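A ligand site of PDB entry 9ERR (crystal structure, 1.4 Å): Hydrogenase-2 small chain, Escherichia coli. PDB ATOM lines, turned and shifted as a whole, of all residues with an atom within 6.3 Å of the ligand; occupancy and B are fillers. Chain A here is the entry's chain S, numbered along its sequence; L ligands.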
ATOM      1  N   ILE A 190      21.726  17.721  -1.481  1.00  0.00           N
ATOM      2  CA  ILE A 190      21.437  18.941  -2.192  1.00  0.00           C
ATOM      3  C   ILE A 190      22.724  19.749  -2.397  1.00  0.00           C
ATOM      4  O   ILE A 190      22.979  20.250  -3.494  1.00  0.00           O
ATOM      5  CB  ILE A 190      20.328  19.765  -1.477  1.00  0.00           C
ATOM      6  CG1 ILE A 190      19.000  19.019  -1.597  1.00  0.00           C
ATOM      7  CG2 ILE A 190      20.268  21.197  -1.966  1.00  0.00           C
ATOM      8  CD1 ILE A 190      17.907  19.580  -0.669  1.00  0.00           C
ATOM      9  N   HIS A 191      23.560  19.834  -1.360  1.00  0.00           N
ATOM     10  CA  HIS A 191      24.810  20.577  -1.460  1.00  0.00           C
ATOM     11  C   HIS A 191      25.816  19.989  -2.462  1.00  0.00           C
ATOM     12  O   HIS A 191      26.741  20.669  -2.869  1.00  0.00           O
ATOM     13  CB  HIS A 191      25.456  20.547  -0.074  1.00  0.00           C
ATOM     14  CG  HIS A 191      26.727  21.306   0.122  1.00  0.00           C
ATOM     15  ND1 HIS A 191      26.826  22.677   0.191  1.00  0.00           N
ATOM     16  CD2 HIS A 191      27.985  20.809   0.380  1.00  0.00           C
ATOM     17  CE1 HIS A 191      28.094  23.001   0.449  1.00  0.00           C
ATOM     18  NE2 HIS A 191      28.814  21.904   0.533  1.00  0.00           N
ATOM     19  N   GLU A 192      25.660  18.695  -2.791  1.00  0.00           N
ATOM     20  CA  GLU A 192      26.543  18.068  -3.772  1.00  0.00           C
ATOM     21  C   GLU A 192      25.975  18.229  -5.185  1.00  0.00           C
ATOM     22  O   GLU A 192      26.522  17.617  -6.135  1.00  0.00           O
ATOM     23  CB  GLU A 192      26.846  16.616  -3.435  1.00  0.00           C
ATOM     24  CG  GLU A 192      27.687  16.443  -2.166  1.00  0.00           C
ATOM     25  CD  GLU A 192      29.013  17.166  -2.258  1.00  0.00           C
ATOM     26  OE1 GLU A 192      29.339  18.003  -1.387  1.00  0.00           O
ATOM     27  OE2 GLU A 192      29.687  16.975  -3.243  1.00  0.00           O
ATOM     28  N   CYS A 194      24.334  21.734  -5.865  1.00  0.00           N
ATOM     29  CA  CYS A 194      23.760  23.069  -5.665  1.00  0.00           C
ATOM     30  C   CYS A 194      24.519  24.101  -6.468  1.00  0.00           C
ATOM     31  O   CYS A 194      25.766  24.180  -6.355  1.00  0.00           O
ATOM     32  CB  CYS A 194      23.825  23.456  -4.197  1.00  0.00           C
ATOM     33  SG  CYS A 194      23.156  25.106  -3.860  1.00  0.00           S
ATOM     34  N   GLU A 195      23.803  24.996  -7.155  1.00  0.00           N
ATOM     35  CA  GLU A 195      24.423  25.985  -8.009  1.00  0.00           C
ATOM     36  C   GLU A 195      25.117  27.102  -7.246  1.00  0.00           C
ATOM     37  O   GLU A 195      25.841  27.906  -7.860  1.00  0.00           O
ATOM     38  CB  GLU A 195      23.380  26.535  -8.976  1.00  0.00           C
ATOM     39  CG  GLU A 195      22.271  27.414  -8.368  1.00  0.00           C
ATOM     40  CD  GLU A 195      21.055  26.696  -7.780  1.00  0.00           C
ATOM     41  OE1 GLU A 195      21.109  25.470  -7.572  1.00  0.00           O
ATOM     42  OE2 GLU A 195      20.024  27.419  -7.560  1.00  0.00           O
ATOM     43  N   ARG A 196      24.945  27.156  -5.914  1.00  0.00           N
ATOM     44  CA  ARG A 196      25.646  28.141  -5.107  1.00  0.00           C
ATOM     45  C   ARG A 196      26.908  27.546  -4.507  1.00  0.00           C
ATOM     46  O   ARG A 196      27.590  28.261  -3.777  1.00  0.00           O
ATOM     47  CB  ARG A 196      24.758  28.744  -4.025  1.00  0.00           C
ATOM     48  CG  ARG A 196      23.493  29.342  -4.639  1.00  0.00           C
ATOM     49  CD  ARG A 196      22.734  30.289  -3.743  1.00  0.00           C
ATOM     50  NE  ARG A 196      21.605  30.874  -4.466  1.00  0.00           N
ATOM     51  CZ  ARG A 196      20.952  31.960  -4.086  1.00  0.00           C
ATOM     52  NH1 ARG A 196      21.241  32.551  -2.947  1.00  0.00           N
ATOM     53  NH2 ARG A 196      19.995  32.438  -4.859  1.00  0.00           N
ATOM     54  N   ARG A 197      27.247  26.299  -4.848  1.00  0.00           N
ATOM     55  CA  ARG A 197      28.493  25.719  -4.315  1.00  0.00           C
ATOM     56  C   ARG A 197      29.711  26.585  -4.647  1.00  0.00           C
ATOM     57  O   ARG A 197      30.638  26.668  -3.818  1.00  0.00           O
ATOM     58  CB  ARG A 197      28.682  24.309  -4.863  1.00  0.00           C
ATOM     59  CG  ARG A 197      29.976  23.645  -4.405  1.00  0.00           C
ATOM     60  CD  ARG A 197      30.054  23.512  -2.899  1.00  0.00           C
ATOM     61  NE  ARG A 197      31.158  22.675  -2.470  1.00  0.00           N
ATOM     62  CZ  ARG A 197      31.133  21.350  -2.421  1.00  0.00           C
ATOM     63  NH1 ARG A 197      29.996  20.686  -2.472  1.00  0.00           N
ATOM     64  NH2 ARG A 197      32.271  20.687  -2.304  1.00  0.00           N
ATOM     65  N   PRO A 198      29.848  27.197  -5.840  1.00  0.00           N
ATOM     66  CA  PRO A 198      31.011  28.067  -6.061  1.00  0.00           C
ATOM     67  C   PRO A 198      31.190  29.151  -4.982  1.00  0.00           C
ATOM     68  O   PRO A 198      32.338  29.524  -4.595  1.00  0.00           O
ATOM     69  CB  PRO A 198      30.696  28.703  -7.415  1.00  0.00           C
ATOM     70  CG  PRO A 198      29.827  27.686  -8.144  1.00  0.00           C
ATOM     71  CD  PRO A 198      28.970  27.106  -7.039  1.00  0.00           C
ATOM     72  N   PHE A 200      30.003  29.046  -1.842  1.00  0.00           N
ATOM     73  CA  PHE A 200      30.452  28.301  -0.671  1.00  0.00           C
ATOM     74  C   PHE A 200      31.974  28.163  -0.702  1.00  0.00           C
ATOM     75  O   PHE A 200      32.665  28.451   0.281  1.00  0.00           O
ATOM     76  CB  PHE A 200      29.725  26.965  -0.611  1.00  0.00           C
ATOM     77  CG  PHE A 200      30.142  26.114   0.574  1.00  0.00           C
ATOM     78  CD1 PHE A 200      31.203  25.252   0.472  1.00  0.00           C
ATOM     79  CD2 PHE A 200      29.431  26.154   1.765  1.00  0.00           C
ATOM     80  CE1 PHE A 200      31.603  24.467   1.542  1.00  0.00           C
ATOM     81  CE2 PHE A 200      29.827  25.367   2.843  1.00  0.00           C
ATOM     82  CZ  PHE A 200      30.877  24.470   2.714  1.00  0.00           C
ATOM     83  N   PHE A 205      29.263  34.447   1.262  1.00  0.00           N
ATOM     84  CA  PHE A 205      28.112  34.043   2.052  1.00  0.00           C
ATOM     85  C   PHE A 205      27.223  35.253   2.360  1.00  0.00           C
ATOM     86  O   PHE A 205      27.678  36.323   2.716  1.00  0.00           O
ATOM     87  CB  PHE A 205      28.563  33.457   3.384  1.00  0.00           C
ATOM     88  CG  PHE A 205      29.409  32.217   3.295  1.00  0.00           C
ATOM     89  CD1 PHE A 205      28.891  31.023   2.845  1.00  0.00           C
ATOM     90  CD2 PHE A 205      30.731  32.221   3.752  1.00  0.00           C
ATOM     91  CE1 PHE A 205      29.604  29.857   2.871  1.00  0.00           C
ATOM     92  CE2 PHE A 205      31.467  31.057   3.721  1.00  0.00           C
ATOM     93  CZ  PHE A 205      30.936  29.872   3.276  1.00  0.00           C
ATOM     94  N   TRP A 218      24.470  34.765  -3.243  1.00  0.00           N
ATOM     95  CA  TRP A 218      25.570  34.009  -2.677  1.00  0.00           C
ATOM     96  C   TRP A 218      25.042  32.841  -1.833  1.00  0.00           C
ATOM     97  O   TRP A 218      23.842  32.662  -1.636  1.00  0.00           O
ATOM     98  CB  TRP A 218      26.460  34.918  -1.828  1.00  0.00           C
ATOM     99  CG  TRP A 218      27.313  35.860  -2.629  1.00  0.00           C
ATOM    100  CD1 TRP A 218      27.418  35.972  -3.976  1.00  0.00           C
ATOM    101  CD2 TRP A 218      28.243  36.824  -2.068  1.00  0.00           C
ATOM    102  NE1 TRP A 218      28.307  36.962  -4.306  1.00  0.00           N
ATOM    103  CE2 TRP A 218      28.837  37.484  -3.151  1.00  0.00           C
ATOM    104  CE3 TRP A 218      28.630  37.166  -0.770  1.00  0.00           C
ATOM    105  CZ2 TRP A 218      29.806  38.480  -2.994  1.00  0.00           C
ATOM    106  CZ3 TRP A 218      29.611  38.128  -0.600  1.00  0.00           C
ATOM    107  CH2 TRP A 218      30.180  38.782  -1.701  1.00  0.00           C
ATOM    108  N   CYS A 219      25.970  32.016  -1.344  1.00  0.00           N
ATOM    109  CA  CYS A 219      25.623  30.806  -0.612  1.00  0.00           C
ATOM    110  C   CYS A 219      24.938  31.166   0.709  1.00  0.00           C
ATOM    111  O   CYS A 219      25.252  32.184   1.326  1.00  0.00           O
ATOM    112  CB  CYS A 219      26.862  29.953  -0.368  1.00  0.00           C
ATOM    113  SG  CYS A 219      26.704  28.588   0.798  1.00  0.00           S
ATOM    114  N   LEU A 220      23.969  30.319   1.120  1.00  0.00           N
ATOM    115  CA  LEU A 220      23.134  30.568   2.283  1.00  0.00           C
ATOM    116  C   LEU A 220      23.554  29.713   3.481  1.00  0.00           C
ATOM    117  O   LEU A 220      22.801  29.595   4.461  1.00  0.00           O
ATOM    118  CB  LEU A 220      21.668  30.342   1.886  1.00  0.00           C
ATOM    119  CG  LEU A 220      21.188  31.111   0.653  1.00  0.00           C
ATOM    120  CD1 LEU A 220      19.683  30.874   0.434  1.00  0.00           C
ATOM    121  CD2 LEU A 220      21.477  32.581   0.758  1.00  0.00           C
ATOM    122  N   TYR A 221      24.755  29.117   3.449  1.00  0.00           N
ATOM    123  CA  TYR A 221      25.228  28.251   4.521  1.00  0.00           C
ATOM    124  C   TYR A 221      25.108  28.954   5.886  1.00  0.00           C
ATOM    125  O   TYR A 221      24.609  28.351   6.862  1.00  0.00           O
ATOM    126  CB  TYR A 221      26.713  27.842   4.327  1.00  0.00           C
ATOM    127  CG  TYR A 221      27.199  26.954   5.451  1.00  0.00           C
ATOM    128  CD1 TYR A 221      26.758  25.674   5.573  1.00  0.00           C
ATOM    129  CD2 TYR A 221      27.975  27.492   6.476  1.00  0.00           C
ATOM    130  CE1 TYR A 221      27.142  24.862   6.626  1.00  0.00           C
ATOM    131  CE2 TYR A 221      28.328  26.721   7.567  1.00  0.00           C
ATOM    132  CZ  TYR A 221      27.901  25.411   7.642  1.00  0.00           C
ATOM    133  OH  TYR A 221      28.218  24.649   8.737  1.00  0.00           O
ATOM    134  N   HIS A 222      25.606  30.189   5.971  1.00  0.00           N
ATOM    135  CA  HIS A 222      25.621  30.929   7.238  1.00  0.00           C
ATOM    136  C   HIS A 222      24.249  31.465   7.655  1.00  0.00           C
ATOM    137  O   HIS A 222      24.149  31.977   8.781  1.00  0.00           O
ATOM    138  CB  HIS A 222      26.720  32.000   7.254  1.00  0.00           C
ATOM    139  CG  HIS A 222      28.038  31.353   7.502  1.00  0.00           C
ATOM    140  ND1 HIS A 222      28.373  30.839   8.729  1.00  0.00           N
ATOM    141  CD2 HIS A 222      29.091  31.102   6.696  1.00  0.00           C
ATOM    142  CE1 HIS A 222      29.570  30.253   8.648  1.00  0.00           C
ATOM    143  NE2 HIS A 222      30.051  30.413   7.407  1.00  0.00           N
ATOM    144  N   CYS A 225      21.537  26.982   5.938  1.00  0.00           N
ATOM    145  CA  CYS A 225      21.192  26.042   4.885  1.00  0.00           C
ATOM    146  C   CYS A 225      21.538  24.606   5.289  1.00  0.00           C
ATOM    147  O   CYS A 225      22.684  24.302   5.632  1.00  0.00           O
ATOM    148  CB  CYS A 225      21.844  26.475   3.589  1.00  0.00           C
ATOM    149  SG  CYS A 225      21.311  25.429   2.209  1.00  0.00           S
ATOM    150  N   LYS A 226      20.573  23.700   5.144  1.00  0.00           N
ATOM    151  CA  LYS A 226      20.725  22.290   5.504  1.00  0.00           C
ATOM    152  C   LYS A 226      21.048  21.437   4.280  1.00  0.00           C
ATOM    153  O   LYS A 226      21.113  20.197   4.371  1.00  0.00           O
ATOM    154  CB  LYS A 226      19.495  21.795   6.233  1.00  0.00           C
ATOM    155  CG  LYS A 226      19.130  22.582   7.475  1.00  0.00           C
ATOM    156  CD  LYS A 226      20.271  22.697   8.461  1.00  0.00           C
ATOM    157  CE  LYS A 226      19.912  23.308   9.797  1.00  0.00           C
ATOM    158  NZ  LYS A 226      19.172  24.589   9.624  1.00  0.00           N
ATOM    159  N   GLY A 227      21.319  22.090   3.146  1.00  0.00           N
ATOM    160  CA  GLY A 227      21.734  21.371   1.929  1.00  0.00           C
ATOM    161  C   GLY A 227      22.859  20.366   2.197  1.00  0.00           C
ATOM    162  O   GLY A 227      22.859  19.259   1.649  1.00  0.00           O
ATOM    163  N   PRO A 228      23.847  20.715   3.033  1.00  0.00           N
ATOM    164  CA  PRO A 228      24.923  19.762   3.294  1.00  0.00           C
ATOM    165  C   PRO A 228      24.534  18.452   3.962  1.00  0.00           C
ATOM    166  O   PRO A 228      25.333  17.508   3.965  1.00  0.00           O
ATOM    167  CB  PRO A 228      25.932  20.566   4.121  1.00  0.00           C
ATOM    168  CG  PRO A 228      25.630  22.020   3.821  1.00  0.00           C
ATOM    169  CD  PRO A 228      24.128  22.072   3.554  1.00  0.00           C
ATOM    170  N   TRP A 246      13.221  27.107  -6.249  1.00  0.00           N
ATOM    171  CA  TRP A 246      13.354  26.287  -5.055  1.00  0.00           C
ATOM    172  C   TRP A 246      13.749  27.208  -3.914  1.00  0.00           C
ATOM    173  O   TRP A 246      14.054  28.390  -4.159  1.00  0.00           O
ATOM    174  CB  TRP A 246      14.349  25.128  -5.259  1.00  0.00           C
ATOM    175  CG  TRP A 246      15.823  25.449  -5.415  1.00  0.00           C
ATOM    176  CD1 TRP A 246      16.464  26.043  -6.472  1.00  0.00           C
ATOM    177  CD2 TRP A 246      16.868  25.050  -4.482  1.00  0.00           C
ATOM    178  NE1 TRP A 246      17.822  26.048  -6.247  1.00  0.00           N
ATOM    179  CE2 TRP A 246      18.098  25.428  -5.059  1.00  0.00           C
ATOM    180  CE3 TRP A 246      16.881  24.374  -3.258  1.00  0.00           C
ATOM    181  CZ2 TRP A 246      19.322  25.181  -4.411  1.00  0.00           C
ATOM    182  CZ3 TRP A 246      18.080  24.100  -2.632  1.00  0.00           C
ATOM    183  CH2 TRP A 246      19.282  24.464  -3.242  1.00  0.00           C
ATOM    184  N   VAL A 248      16.303  27.897  -1.899  1.00  0.00           N
ATOM    185  CA  VAL A 248      17.586  28.602  -1.963  1.00  0.00           C
ATOM    186  C   VAL A 248      17.606  29.603  -3.124  1.00  0.00           C
ATOM    187  O   VAL A 248      18.026  30.748  -2.966  1.00  0.00           O
ATOM    188  CB  VAL A 248      18.727  27.576  -2.054  1.00  0.00           C
ATOM    189  CG1 VAL A 248      20.009  28.220  -2.532  1.00  0.00           C
ATOM    190  CG2 VAL A 248      18.902  26.842  -0.740  1.00  0.00           C
ATOM    191  N   PRO A 253      17.424  29.579   3.086  1.00  0.00           N
ATOM    192  CA  PRO A 253      18.125  28.310   3.249  1.00  0.00           C
ATOM    193  C   PRO A 253      17.187  27.116   3.160  1.00  0.00           C
ATOM    194  O   PRO A 253      16.029  27.208   3.570  1.00  0.00           O
ATOM    195  CB  PRO A 253      18.746  28.441   4.646  1.00  0.00           C
ATOM    196  CG  PRO A 253      17.944  29.527   5.330  1.00  0.00           C
ATOM    197  CD  PRO A 253      17.600  30.497   4.220  1.00  0.00           C
ATOM    198  N   CYS A 254      17.732  25.998   2.679  1.00  0.00           N
ATOM    199  CA  CYS A 254      17.119  24.710   2.908  1.00  0.00           C
ATOM    200  C   CYS A 254      17.008  24.488   4.418  1.00  0.00           C
ATOM    201  O   CYS A 254      17.942  24.806   5.163  1.00  0.00           O
ATOM    202  CB  CYS A 254      17.919  23.575   2.258  1.00  0.00           C
ATOM    203  SG  CYS A 254      17.364  21.891   2.609  1.00  0.00           S
HETATM  204 FE1  LIG L   1      25.388  26.903   0.022  1.00  0.00          FE
HETATM  205 FE2  LIG L   1      23.154  25.494   0.821  1.00  0.00          FE
HETATM  206 FE3  LIG L   1      25.420  24.156   0.065  1.00  0.00          FE
HETATM  207 FE4  LIG L   1      23.933  25.439  -1.795  1.00  0.00          FE
HETATM  208  S1  LIG L   1      23.302  23.631  -0.493  1.00  0.00           S
HETATM  209  S2  LIG L   1      26.213  25.555  -1.632  1.00  0.00           S
HETATM  210  S3  LIG L   1      23.263  27.297  -0.608  1.00  0.00           S
HETATM  211  S4  LIG L   1      25.158  25.497   1.858  1.00  0.00           S
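ND1 of His 191 is bound to FE3 of the ligand (2.0 Å).
SG of Cys 194 binds FE4 of the ligand.
An iron atom (FE1) of the ligand is bound by the side-chain sulfur of Cys 219, 2.3 Å away.
The side-chain sulfur (SG) of Cys 225 binds an iron atom (FE2) of the ligand, 2.3 Å away.
A sulfur (S2) of the ligand sits close to the backbone NH (N) of Arg 197 (3.5 Å).
N of Leu 220 lies close to S3 of the ligand (3.6 Å).
The backbone carbonyl oxygen (O) of Gly 227 lies within hydrogen-bond range of the backbone NH (N) of His 191, at 3.1 Å.
The side-chain sulfur of Cys 194 sits close to the backbone NH of Arg 196 (3.4 Å).
O of Leu 220 lies within hydrogen-bond range of N of Cys 225, 3.3 Å away.
N of Gly 227 sits close to SG of Cys 225 (3.5 Å).
The side-chain sulfur (SG) of Cys 225 lies close to the backbone NH (N) of Cys 254 (3.7 Å).
The side-chain carboxylate (OE1) of Glu 192 is in salt-bridge range of the guanidinium group (NH1) of Arg 197 (3.0 Å).
The guanidinium group (NH2) of Arg 196 lies within hydrogen-bond range of the backbone carbonyl oxygen (O) of Val 248 (3.2 Å).
The guanidinium group of Arg 196 sits at hydrogen-bond distance from the backbone carbonyl oxygen of Trp 218.
The backbone carbonyl oxygen (O) of Arg 196 lies close to a sulfur (S2) of the ligand (3.7 Å).
Merely in contact with the ligand: Gly 227 (3.7 Å), Tyr 221 (3.7 Å), Val 248 (3.9 Å), Phe 200 (3.9 Å) and Pro 228 (3.96 Å).
Hydrophobic or aromatic side chains that line the ligand: His 191, Phe 200, Tyr 221, Pro 228 and Val 248.
12 residues have an atom within 4 Å of the ligand: His 191, Cys 194, Arg 196, Arg 197, Phe 200, Cys 219, Leu 220, Tyr 221, Cys 225, Gly 227, Pro 228 and Val 248.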
